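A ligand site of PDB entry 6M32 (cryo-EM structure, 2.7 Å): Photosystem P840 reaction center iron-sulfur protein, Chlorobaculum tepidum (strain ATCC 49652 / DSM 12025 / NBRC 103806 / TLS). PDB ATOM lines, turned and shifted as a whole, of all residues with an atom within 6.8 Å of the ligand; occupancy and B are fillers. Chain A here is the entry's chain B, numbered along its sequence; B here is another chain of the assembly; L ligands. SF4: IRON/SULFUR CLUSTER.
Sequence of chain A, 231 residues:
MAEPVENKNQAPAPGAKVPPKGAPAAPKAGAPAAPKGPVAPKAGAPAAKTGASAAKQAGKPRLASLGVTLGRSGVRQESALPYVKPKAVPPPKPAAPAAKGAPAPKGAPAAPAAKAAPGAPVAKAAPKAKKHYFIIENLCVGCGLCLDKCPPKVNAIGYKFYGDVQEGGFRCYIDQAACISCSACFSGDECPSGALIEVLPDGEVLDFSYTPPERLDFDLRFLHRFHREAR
O of Cys 140 sits at hydrogen-bond distance from NH1 of Arg 171 (3.3 Å). The side-chain sulfur (SG) of Cys 172 lies close to the side-chain sulfur (SG) of Cys 140 (3.5 Å). The side-chain sulfur (SG) of Cys 143 sits close to the backbone NH (N) of Leu 145, 3.7 Å away. The side-chain sulfur of Cys 191 sits close to the backbone NH of Leu 196, at 3.8 Å. O of Leu 139 lies within hydrogen-bond range of OG of Ser 193 (3.0 Å). O of Ala 195 lies within hydrogen-bond range of N of Ile 136, at 2.5 Å. The backbone carbonyl oxygen (O) of Gly 142 sits at hydrogen-bond distance from the side-chain hydroxyl (OH) of Tyr 159, at 3.2 Å. The side-chain sulfur (SG) of Cys 172 lies close to the side-chain sulfur (SG) of Cys 146, 3.6 Å away.
Residues that only touch the ligand: Leu 196, Ala 195, Pro 192, Gly 142 and Ile 135. Hydrophobic or aromatic side chains that line the ligand: Ile 135, Val 141, Pro 192, Ala 195 and Leu 196. Within 4 Å of the ligand: Ile 135, Cys 140, Val 141, Gly 142, Cys 143, Gly 144, Cys 146, Cys 172, Cys 191, Pro 192, Ser 193, Ala 195 and Leu 196.
A sulfur (S2) of the ligand sits close to the backbone NH (N) of Cys 146 (3.6 Å). SG of Cys 140 is bound to FE2 of the ligand (2.5 Å). A sulfur (S3) of the ligand lies close to the backbone NH (N) of Cys 143 (3.6 Å). The side-chain hydroxyl (OG) of Ser 193 sits close to a sulfur (S4) of the ligand, 3.4 Å away. FE4 of the ligand is bound by SG of Cys 146, 2.2 Å away. N of Gly 144 sits close to S3 of the ligand, 3.3 Å away. S4 of the ligand sits close to N of Val 141 (3.6 Å). An iron atom (FE1) of the ligand is bound by the side-chain sulfur (SG) of Cys 143 (2.2 Å). The side-chain sulfur (SG) of Cys 172 lies close to a sulfur (S3) of the ligand (3.0 Å). SG of Cys 191 binds FE3 of the ligand, 2.2 Å away.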
ATOM      1  N   ILE A 135      16.368  23.272  34.904  1.00  0.00           N
ATOM      2  CA  ILE A 135      16.018  24.032  33.698  1.00  0.00           C
ATOM      3  C   ILE A 135      15.025  23.249  32.850  1.00  0.00           C
ATOM      4  O   ILE A 135      15.225  22.065  32.583  1.00  0.00           O
ATOM      5  CB  ILE A 135      17.273  24.386  32.891  1.00  0.00           C
ATOM      6  CG1 ILE A 135      18.082  25.492  33.550  1.00  0.00           C
ATOM      7  CG2 ILE A 135      16.897  24.795  31.477  1.00  0.00           C
ATOM      8  CD1 ILE A 135      19.344  25.846  32.798  1.00  0.00           C
ATOM      9  N   ILE A 136      13.946  23.926  32.418  1.00  0.00           N
ATOM     10  CA  ILE A 136      12.980  23.354  31.494  1.00  0.00           C
ATOM     11  C   ILE A 136      13.568  23.379  30.096  1.00  0.00           C
ATOM     12  O   ILE A 136      14.144  24.389  29.672  1.00  0.00           O
ATOM     13  CB  ILE A 136      11.651  24.134  31.530  1.00  0.00           C
ATOM     14  CG1 ILE A 136      10.933  23.943  32.859  1.00  0.00           C
ATOM     15  CG2 ILE A 136      10.728  23.682  30.401  1.00  0.00           C
ATOM     16  CD1 ILE A 136       9.656  24.745  32.974  1.00  0.00           C
ATOM     17  N   LEU A 139      11.031  25.477  27.146  1.00  0.00           N
ATOM     18  CA  LEU A 139      10.885  26.923  27.284  1.00  0.00           C
ATOM     19  C   LEU A 139      12.186  27.693  27.136  1.00  0.00           C
ATOM     20  O   LEU A 139      12.139  28.901  26.874  1.00  0.00           O
ATOM     21  CB  LEU A 139      10.280  27.278  28.652  1.00  0.00           C
ATOM     22  CG  LEU A 139       8.796  27.072  28.871  1.00  0.00           C
ATOM     23  CD1 LEU A 139       8.418  27.505  30.269  1.00  0.00           C
ATOM     24  CD2 LEU A 139       8.009  27.877  27.857  1.00  0.00           C
ATOM     25  N   CYS A 140      13.338  27.048  27.283  1.00  0.00           N
ATOM     26  CA  CYS A 140      14.590  27.776  27.262  1.00  0.00           C
ATOM     27  C   CYS A 140      14.803  28.447  25.915  1.00  0.00           C
ATOM     28  O   CYS A 140      14.396  27.936  24.863  1.00  0.00           O
ATOM     29  CB  CYS A 140      15.764  26.852  27.572  1.00  0.00           C
ATOM     30  SG  CYS A 140      17.355  27.703  27.569  1.00  0.00           S
ATOM     31  N   VAL A 141      15.440  29.613  25.952  1.00  0.00           N
ATOM     32  CA  VAL A 141      15.824  30.322  24.742  1.00  0.00           C
ATOM     33  C   VAL A 141      17.325  30.448  24.585  1.00  0.00           C
ATOM     34  O   VAL A 141      17.794  30.921  23.538  1.00  0.00           O
ATOM     35  CB  VAL A 141      15.172  31.717  24.667  1.00  0.00           C
ATOM     36  CG1 VAL A 141      13.663  31.588  24.512  1.00  0.00           C
ATOM     37  CG2 VAL A 141      15.508  32.527  25.888  1.00  0.00           C
ATOM     38  N   GLY A 142      18.109  30.043  25.582  1.00  0.00           N
ATOM     39  CA  GLY A 142      19.548  30.048  25.461  1.00  0.00           C
ATOM     40  C   GLY A 142      20.226  31.376  25.727  1.00  0.00           C
ATOM     41  O   GLY A 142      21.356  31.587  25.277  1.00  0.00           O
ATOM     42  N   CYS A 143      19.570  32.276  26.455  1.00  0.00           N
ATOM     43  CA  CYS A 143      20.187  33.562  26.735  1.00  0.00           C
ATOM     44  C   CYS A 143      21.467  33.415  27.545  1.00  0.00           C
ATOM     45  O   CYS A 143      22.370  34.260  27.442  1.00  0.00           O
ATOM     46  CB  CYS A 143      19.204  34.469  27.471  1.00  0.00           C
ATOM     47  SG  CYS A 143      18.771  33.951  29.134  1.00  0.00           S
ATOM     48  N   GLY A 144      21.590  32.353  28.346  1.00  0.00           N
ATOM     49  CA  GLY A 144      22.808  32.064  29.065  1.00  0.00           C
ATOM     50  C   GLY A 144      22.998  32.809  30.360  1.00  0.00           C
ATOM     51  O   GLY A 144      24.016  32.591  31.036  1.00  0.00           O
ATOM     52  N   LEU A 145      22.063  33.675  30.749  1.00  0.00           N
ATOM     53  CA  LEU A 145      22.181  34.377  32.024  1.00  0.00           C
ATOM     54  C   LEU A 145      22.208  33.414  33.197  1.00  0.00           C
ATOM     55  O   LEU A 145      22.847  33.704  34.211  1.00  0.00           O
ATOM     56  CB  LEU A 145      21.051  35.376  32.185  1.00  0.00           C
ATOM     57  CG  LEU A 145      20.745  36.258  30.980  1.00  0.00           C
ATOM     58  CD1 LEU A 145      19.436  37.000  31.171  1.00  0.00           C
ATOM     59  CD2 LEU A 145      21.878  37.241  30.742  1.00  0.00           C
ATOM     60  N   CYS A 146      21.527  32.276  33.086  1.00  0.00           N
ATOM     61  CA  CYS A 146      21.590  31.254  34.121  1.00  0.00           C
ATOM     62  C   CYS A 146      22.990  30.698  34.288  1.00  0.00           C
ATOM     63  O   CYS A 146      23.407  30.420  35.418  1.00  0.00           O
ATOM     64  CB  CYS A 146      20.629  30.104  33.800  1.00  0.00           C
ATOM     65  SG  CYS A 146      20.884  29.375  32.170  1.00  0.00           S
ATOM     66  N   LEU A 147      23.720  30.520  33.190  1.00  0.00           N
ATOM     67  CA  LEU A 147      25.054  29.951  33.215  1.00  0.00           C
ATOM     68  C   LEU A 147      26.092  30.855  33.871  1.00  0.00           C
ATOM     69  O   LEU A 147      27.090  30.345  34.397  1.00  0.00           O
ATOM     70  CB  LEU A 147      25.473  29.619  31.776  1.00  0.00           C
ATOM     71  CG  LEU A 147      26.749  28.845  31.468  1.00  0.00           C
ATOM     72  CD1 LEU A 147      26.585  28.121  30.156  1.00  0.00           C
ATOM     73  CD2 LEU A 147      27.921  29.800  31.376  1.00  0.00           C
ATOM     74  N   ILE A 157      26.109  23.883  34.400  1.00  0.00           N
ATOM     75  CA  ILE A 157      25.237  24.344  33.334  1.00  0.00           C
ATOM     76  C   ILE A 157      25.981  24.265  32.019  1.00  0.00           C
ATOM     77  O   ILE A 157      27.143  24.680  31.919  1.00  0.00           O
ATOM     78  CB  ILE A 157      24.737  25.777  33.612  1.00  0.00           C
ATOM     79  CG1 ILE A 157      24.078  25.850  34.981  1.00  0.00           C
ATOM     80  CG2 ILE A 157      23.764  26.215  32.529  1.00  0.00           C
ATOM     81  CD1 ILE A 157      23.382  27.155  35.239  1.00  0.00           C
ATOM     82  N   TYR A 159      25.471  23.600  27.316  1.00  0.00           N
ATOM     83  CA  TYR A 159      24.743  23.936  26.092  1.00  0.00           C
ATOM     84  C   TYR A 159      24.474  22.700  25.260  1.00  0.00           C
ATOM     85  O   TYR A 159      25.178  21.697  25.360  1.00  0.00           O
ATOM     86  CB  TYR A 159      25.529  24.952  25.261  1.00  0.00           C
ATOM     87  CG  TYR A 159      25.169  26.391  25.522  1.00  0.00           C
ATOM     88  CD1 TYR A 159      23.967  26.913  25.077  1.00  0.00           C
ATOM     89  CD2 TYR A 159      26.034  27.228  26.206  1.00  0.00           C
ATOM     90  CE1 TYR A 159      23.638  28.233  25.322  1.00  0.00           C
ATOM     91  CE2 TYR A 159      25.721  28.539  26.449  1.00  0.00           C
ATOM     92  CZ  TYR A 159      24.511  29.040  25.998  1.00  0.00           C
ATOM     93  OH  TYR A 159      24.189  30.350  26.235  1.00  0.00           O
ATOM     94  N   PHE A 170      19.788  26.298  20.496  1.00  0.00           N
ATOM     95  CA  PHE A 170      20.947  26.157  21.377  1.00  0.00           C
ATOM     96  C   PHE A 170      20.527  26.198  22.833  1.00  0.00           C
ATOM     97  O   PHE A 170      21.152  26.857  23.667  1.00  0.00           O
ATOM     98  CB  PHE A 170      22.007  27.227  21.097  1.00  0.00           C
ATOM     99  CG  PHE A 170      21.525  28.630  21.273  1.00  0.00           C
ATOM    100  CD1 PHE A 170      20.564  29.169  20.444  1.00  0.00           C
ATOM    101  CD2 PHE A 170      22.065  29.427  22.272  1.00  0.00           C
ATOM    102  CE1 PHE A 170      20.135  30.455  20.608  1.00  0.00           C
ATOM    103  CE2 PHE A 170      21.636  30.722  22.436  1.00  0.00           C
ATOM    104  CZ  PHE A 170      20.667  31.241  21.601  1.00  0.00           C
ATOM    105  N   ARG A 171      19.460  25.479  23.167  1.00  0.00           N
ATOM    106  CA  ARG A 171      18.920  25.525  24.516  1.00  0.00           C
ATOM    107  C   ARG A 171      19.904  24.908  25.514  1.00  0.00           C
ATOM    108  O   ARG A 171      20.590  23.922  25.204  1.00  0.00           O
ATOM    109  CB  ARG A 171      17.569  24.823  24.548  1.00  0.00           C
ATOM    110  CG  ARG A 171      17.635  23.323  24.320  1.00  0.00           C
ATOM    111  CD  ARG A 171      16.235  22.759  24.342  1.00  0.00           C
ATOM    112  NE  ARG A 171      15.468  23.284  23.221  1.00  0.00           N
ATOM    113  CZ  ARG A 171      14.484  24.178  23.316  1.00  0.00           C
ATOM    114  NH1 ARG A 171      14.164  24.692  24.493  1.00  0.00           N
ATOM    115  NH2 ARG A 171      13.847  24.578  22.232  1.00  0.00           N
ATOM    116  N   CYS A 172      19.996  25.498  26.700  1.00  0.00           N
ATOM    117  CA  CYS A 172      20.952  25.070  27.706  1.00  0.00           C
ATOM    118  C   CYS A 172      20.321  24.030  28.635  1.00  0.00           C
ATOM    119  O   CYS A 172      19.151  23.674  28.500  1.00  0.00           O
ATOM    120  CB  CYS A 172      21.460  26.265  28.498  1.00  0.00           C
ATOM    121  SG  CYS A 172      20.183  27.062  29.496  1.00  0.00           S
ATOM    122  N   TYR A 173      21.109  23.555  29.582  1.00  0.00           N
ATOM    123  CA  TYR A 173      20.654  22.512  30.498  1.00  0.00           C
ATOM    124  C   TYR A 173      21.515  22.552  31.759  1.00  0.00           C
ATOM    125  O   TYR A 173      22.555  23.212  31.798  1.00  0.00           O
ATOM    126  CB  TYR A 173      20.702  21.139  29.837  1.00  0.00           C
ATOM    127  CG  TYR A 173      22.102  20.601  29.698  1.00  0.00           C
ATOM    128  CD1 TYR A 173      22.932  21.028  28.681  1.00  0.00           C
ATOM    129  CD2 TYR A 173      22.603  19.665  30.596  1.00  0.00           C
ATOM    130  CE1 TYR A 173      24.217  20.546  28.555  1.00  0.00           C
ATOM    131  CE2 TYR A 173      23.882  19.173  30.478  1.00  0.00           C
ATOM    132  CZ  TYR A 173      24.682  19.618  29.451  1.00  0.00           C
ATOM    133  OH  TYR A 173      25.968  19.136  29.324  1.00  0.00           O
ATOM    134  N   GLU A 190      16.599  36.081  36.803  1.00  0.00           N
ATOM    135  CA  GLU A 190      17.106  36.453  35.489  1.00  0.00           C
ATOM    136  C   GLU A 190      16.432  35.741  34.334  1.00  0.00           C
ATOM    137  O   GLU A 190      16.413  36.264  33.221  1.00  0.00           O
ATOM    138  CB  GLU A 190      18.615  36.200  35.406  1.00  0.00           C
ATOM    139  CG  GLU A 190      19.033  34.735  35.395  1.00  0.00           C
ATOM    140  CD  GLU A 190      19.155  34.127  36.767  1.00  0.00           C
ATOM    141  OE1 GLU A 190      18.637  34.723  37.738  1.00  0.00           O
ATOM    142  OE2 GLU A 190      19.791  33.061  36.876  1.00  0.00           O
ATOM    143  N   CYS A 191      15.888  34.550  34.550  1.00  0.00           N
ATOM    144  CA  CYS A 191      15.337  33.772  33.453  1.00  0.00           C
ATOM    145  C   CYS A 191      14.119  34.483  32.872  1.00  0.00           C
ATOM    146  O   CYS A 191      13.188  34.802  33.622  1.00  0.00           O
ATOM    147  CB  CYS A 191      14.952  32.369  33.916  1.00  0.00           C
ATOM    148  SG  CYS A 191      14.547  31.245  32.556  1.00  0.00           S
ATOM    149  N   PRO A 192      14.096  34.765  31.570  1.00  0.00           N
ATOM    150  CA  PRO A 192      12.949  35.459  30.981  1.00  0.00           C
ATOM    151  C   PRO A 192      11.860  34.554  30.437  1.00  0.00           C
ATOM    152  O   PRO A 192      10.767  35.050  30.129  1.00  0.00           O
ATOM    153  CB  PRO A 192      13.595  36.278  29.854  1.00  0.00           C
ATOM    154  CG  PRO A 192      15.008  35.741  29.699  1.00  0.00           C
ATOM    155  CD  PRO A 192      15.167  34.561  30.589  1.00  0.00           C
ATOM    156  N   SER A 193      12.100  33.261  30.301  1.00  0.00           N
ATOM    157  CA  SER A 193      11.101  32.339  29.790  1.00  0.00           C
ATOM    158  C   SER A 193      10.445  31.499  30.883  1.00  0.00           C
ATOM    159  O   SER A 193       9.570  30.694  30.563  1.00  0.00           O
ATOM    160  CB  SER A 193      11.724  31.407  28.754  1.00  0.00           C
ATOM    161  OG  SER A 193      12.659  30.535  29.361  1.00  0.00           O
ATOM    162  N   GLY A 194      10.845  31.662  32.139  1.00  0.00           N
ATOM    163  CA  GLY A 194      10.369  30.768  33.169  1.00  0.00           C
ATOM    164  C   GLY A 194      10.844  29.344  32.987  1.00  0.00           C
ATOM    165  O   GLY A 194      10.063  28.405  33.198  1.00  0.00           O
ATOM    166  N   ALA A 195      12.104  29.150  32.604  1.00  0.00           N
ATOM    167  CA  ALA A 195      12.642  27.819  32.385  1.00  0.00           C
ATOM    168  C   ALA A 195      13.311  27.241  33.632  1.00  0.00           C
ATOM    169  O   ALA A 195      13.387  26.014  33.763  1.00  0.00           O
ATOM    170  CB  ALA A 195      13.642  27.831  31.226  1.00  0.00           C
ATOM    171  N   LEU A 196      13.801  28.085  34.529  1.00  0.00           N
ATOM    172  CA  LEU A 196      14.280  27.630  35.831  1.00  0.00           C
ATOM    173  C   LEU A 196      13.094  27.560  36.777  1.00  0.00           C
ATOM    174  O   LEU A 196      12.242  28.468  36.787  1.00  0.00           O
ATOM    175  CB  LEU A 196      15.334  28.574  36.400  1.00  0.00           C
ATOM    176  CG  LEU A 196      16.766  28.526  35.890  1.00  0.00           C
ATOM    177  CD1 LEU A 196      16.857  29.083  34.493  1.00  0.00           C
ATOM    178  CD2 LEU A 196      17.655  29.296  36.820  1.00  0.00           C
ATOM    179  N   LEU B 518       7.928  35.718  27.555  1.00  0.00           N
ATOM    180  CA  LEU B 518       9.220  36.349  27.794  1.00  0.00           C
ATOM    181  C   LEU B 518       9.090  37.501  28.779  1.00  0.00           C
ATOM    182  O   LEU B 518       7.993  37.981  29.070  1.00  0.00           O
ATOM    183  CB  LEU B 518       9.842  36.837  26.473  1.00  0.00           C
ATOM    184  CG  LEU B 518      10.412  35.713  25.594  1.00  0.00           C
ATOM    185  CD1 LEU B 518      10.676  36.156  24.179  1.00  0.00           C
ATOM    186  CD2 LEU B 518      11.665  35.144  26.219  1.00  0.00           C
ATOM    187  N   LEU B 528      18.929  38.935  24.285  1.00  0.00           N
ATOM    188  CA  LEU B 528      18.575  37.602  24.736  1.00  0.00           C
ATOM    189  C   LEU B 528      19.175  36.500  23.882  1.00  0.00           C
ATOM    190  O   LEU B 528      18.953  35.322  24.175  1.00  0.00           O
ATOM    191  CB  LEU B 528      17.049  37.434  24.783  1.00  0.00           C
ATOM    192  CG  LEU B 528      16.343  38.054  25.988  1.00  0.00           C
ATOM    193  CD1 LEU B 528      14.876  37.687  25.987  1.00  0.00           C
ATOM    194  CD2 LEU B 528      17.012  37.596  27.276  1.00  0.00           C
HETATM  195 FE1  SF4 L   1      18.136  31.857  29.560  1.00  0.00          FE
HETATM  196 FE2  SF4 L   1      17.324  29.314  29.464  1.00  0.00          FE
HETATM  197 FE3  SF4 L   1      16.348  30.958  31.387  1.00  0.00          FE
HETATM  198 FE4  SF4 L   1      18.885  30.145  31.506  1.00  0.00          FE
HETATM  199  S1  SF4 L   1      17.058  28.815  31.655  1.00  0.00           S
HETATM  200  S2  SF4 L   1      18.126  32.259  31.799  1.00  0.00           S
HETATM  201  S3  SF4 L   1      19.479  30.016  29.291  1.00  0.00           S
HETATM  202  S4  SF4 L   1      16.041  31.174  29.128  1.00  0.00           S
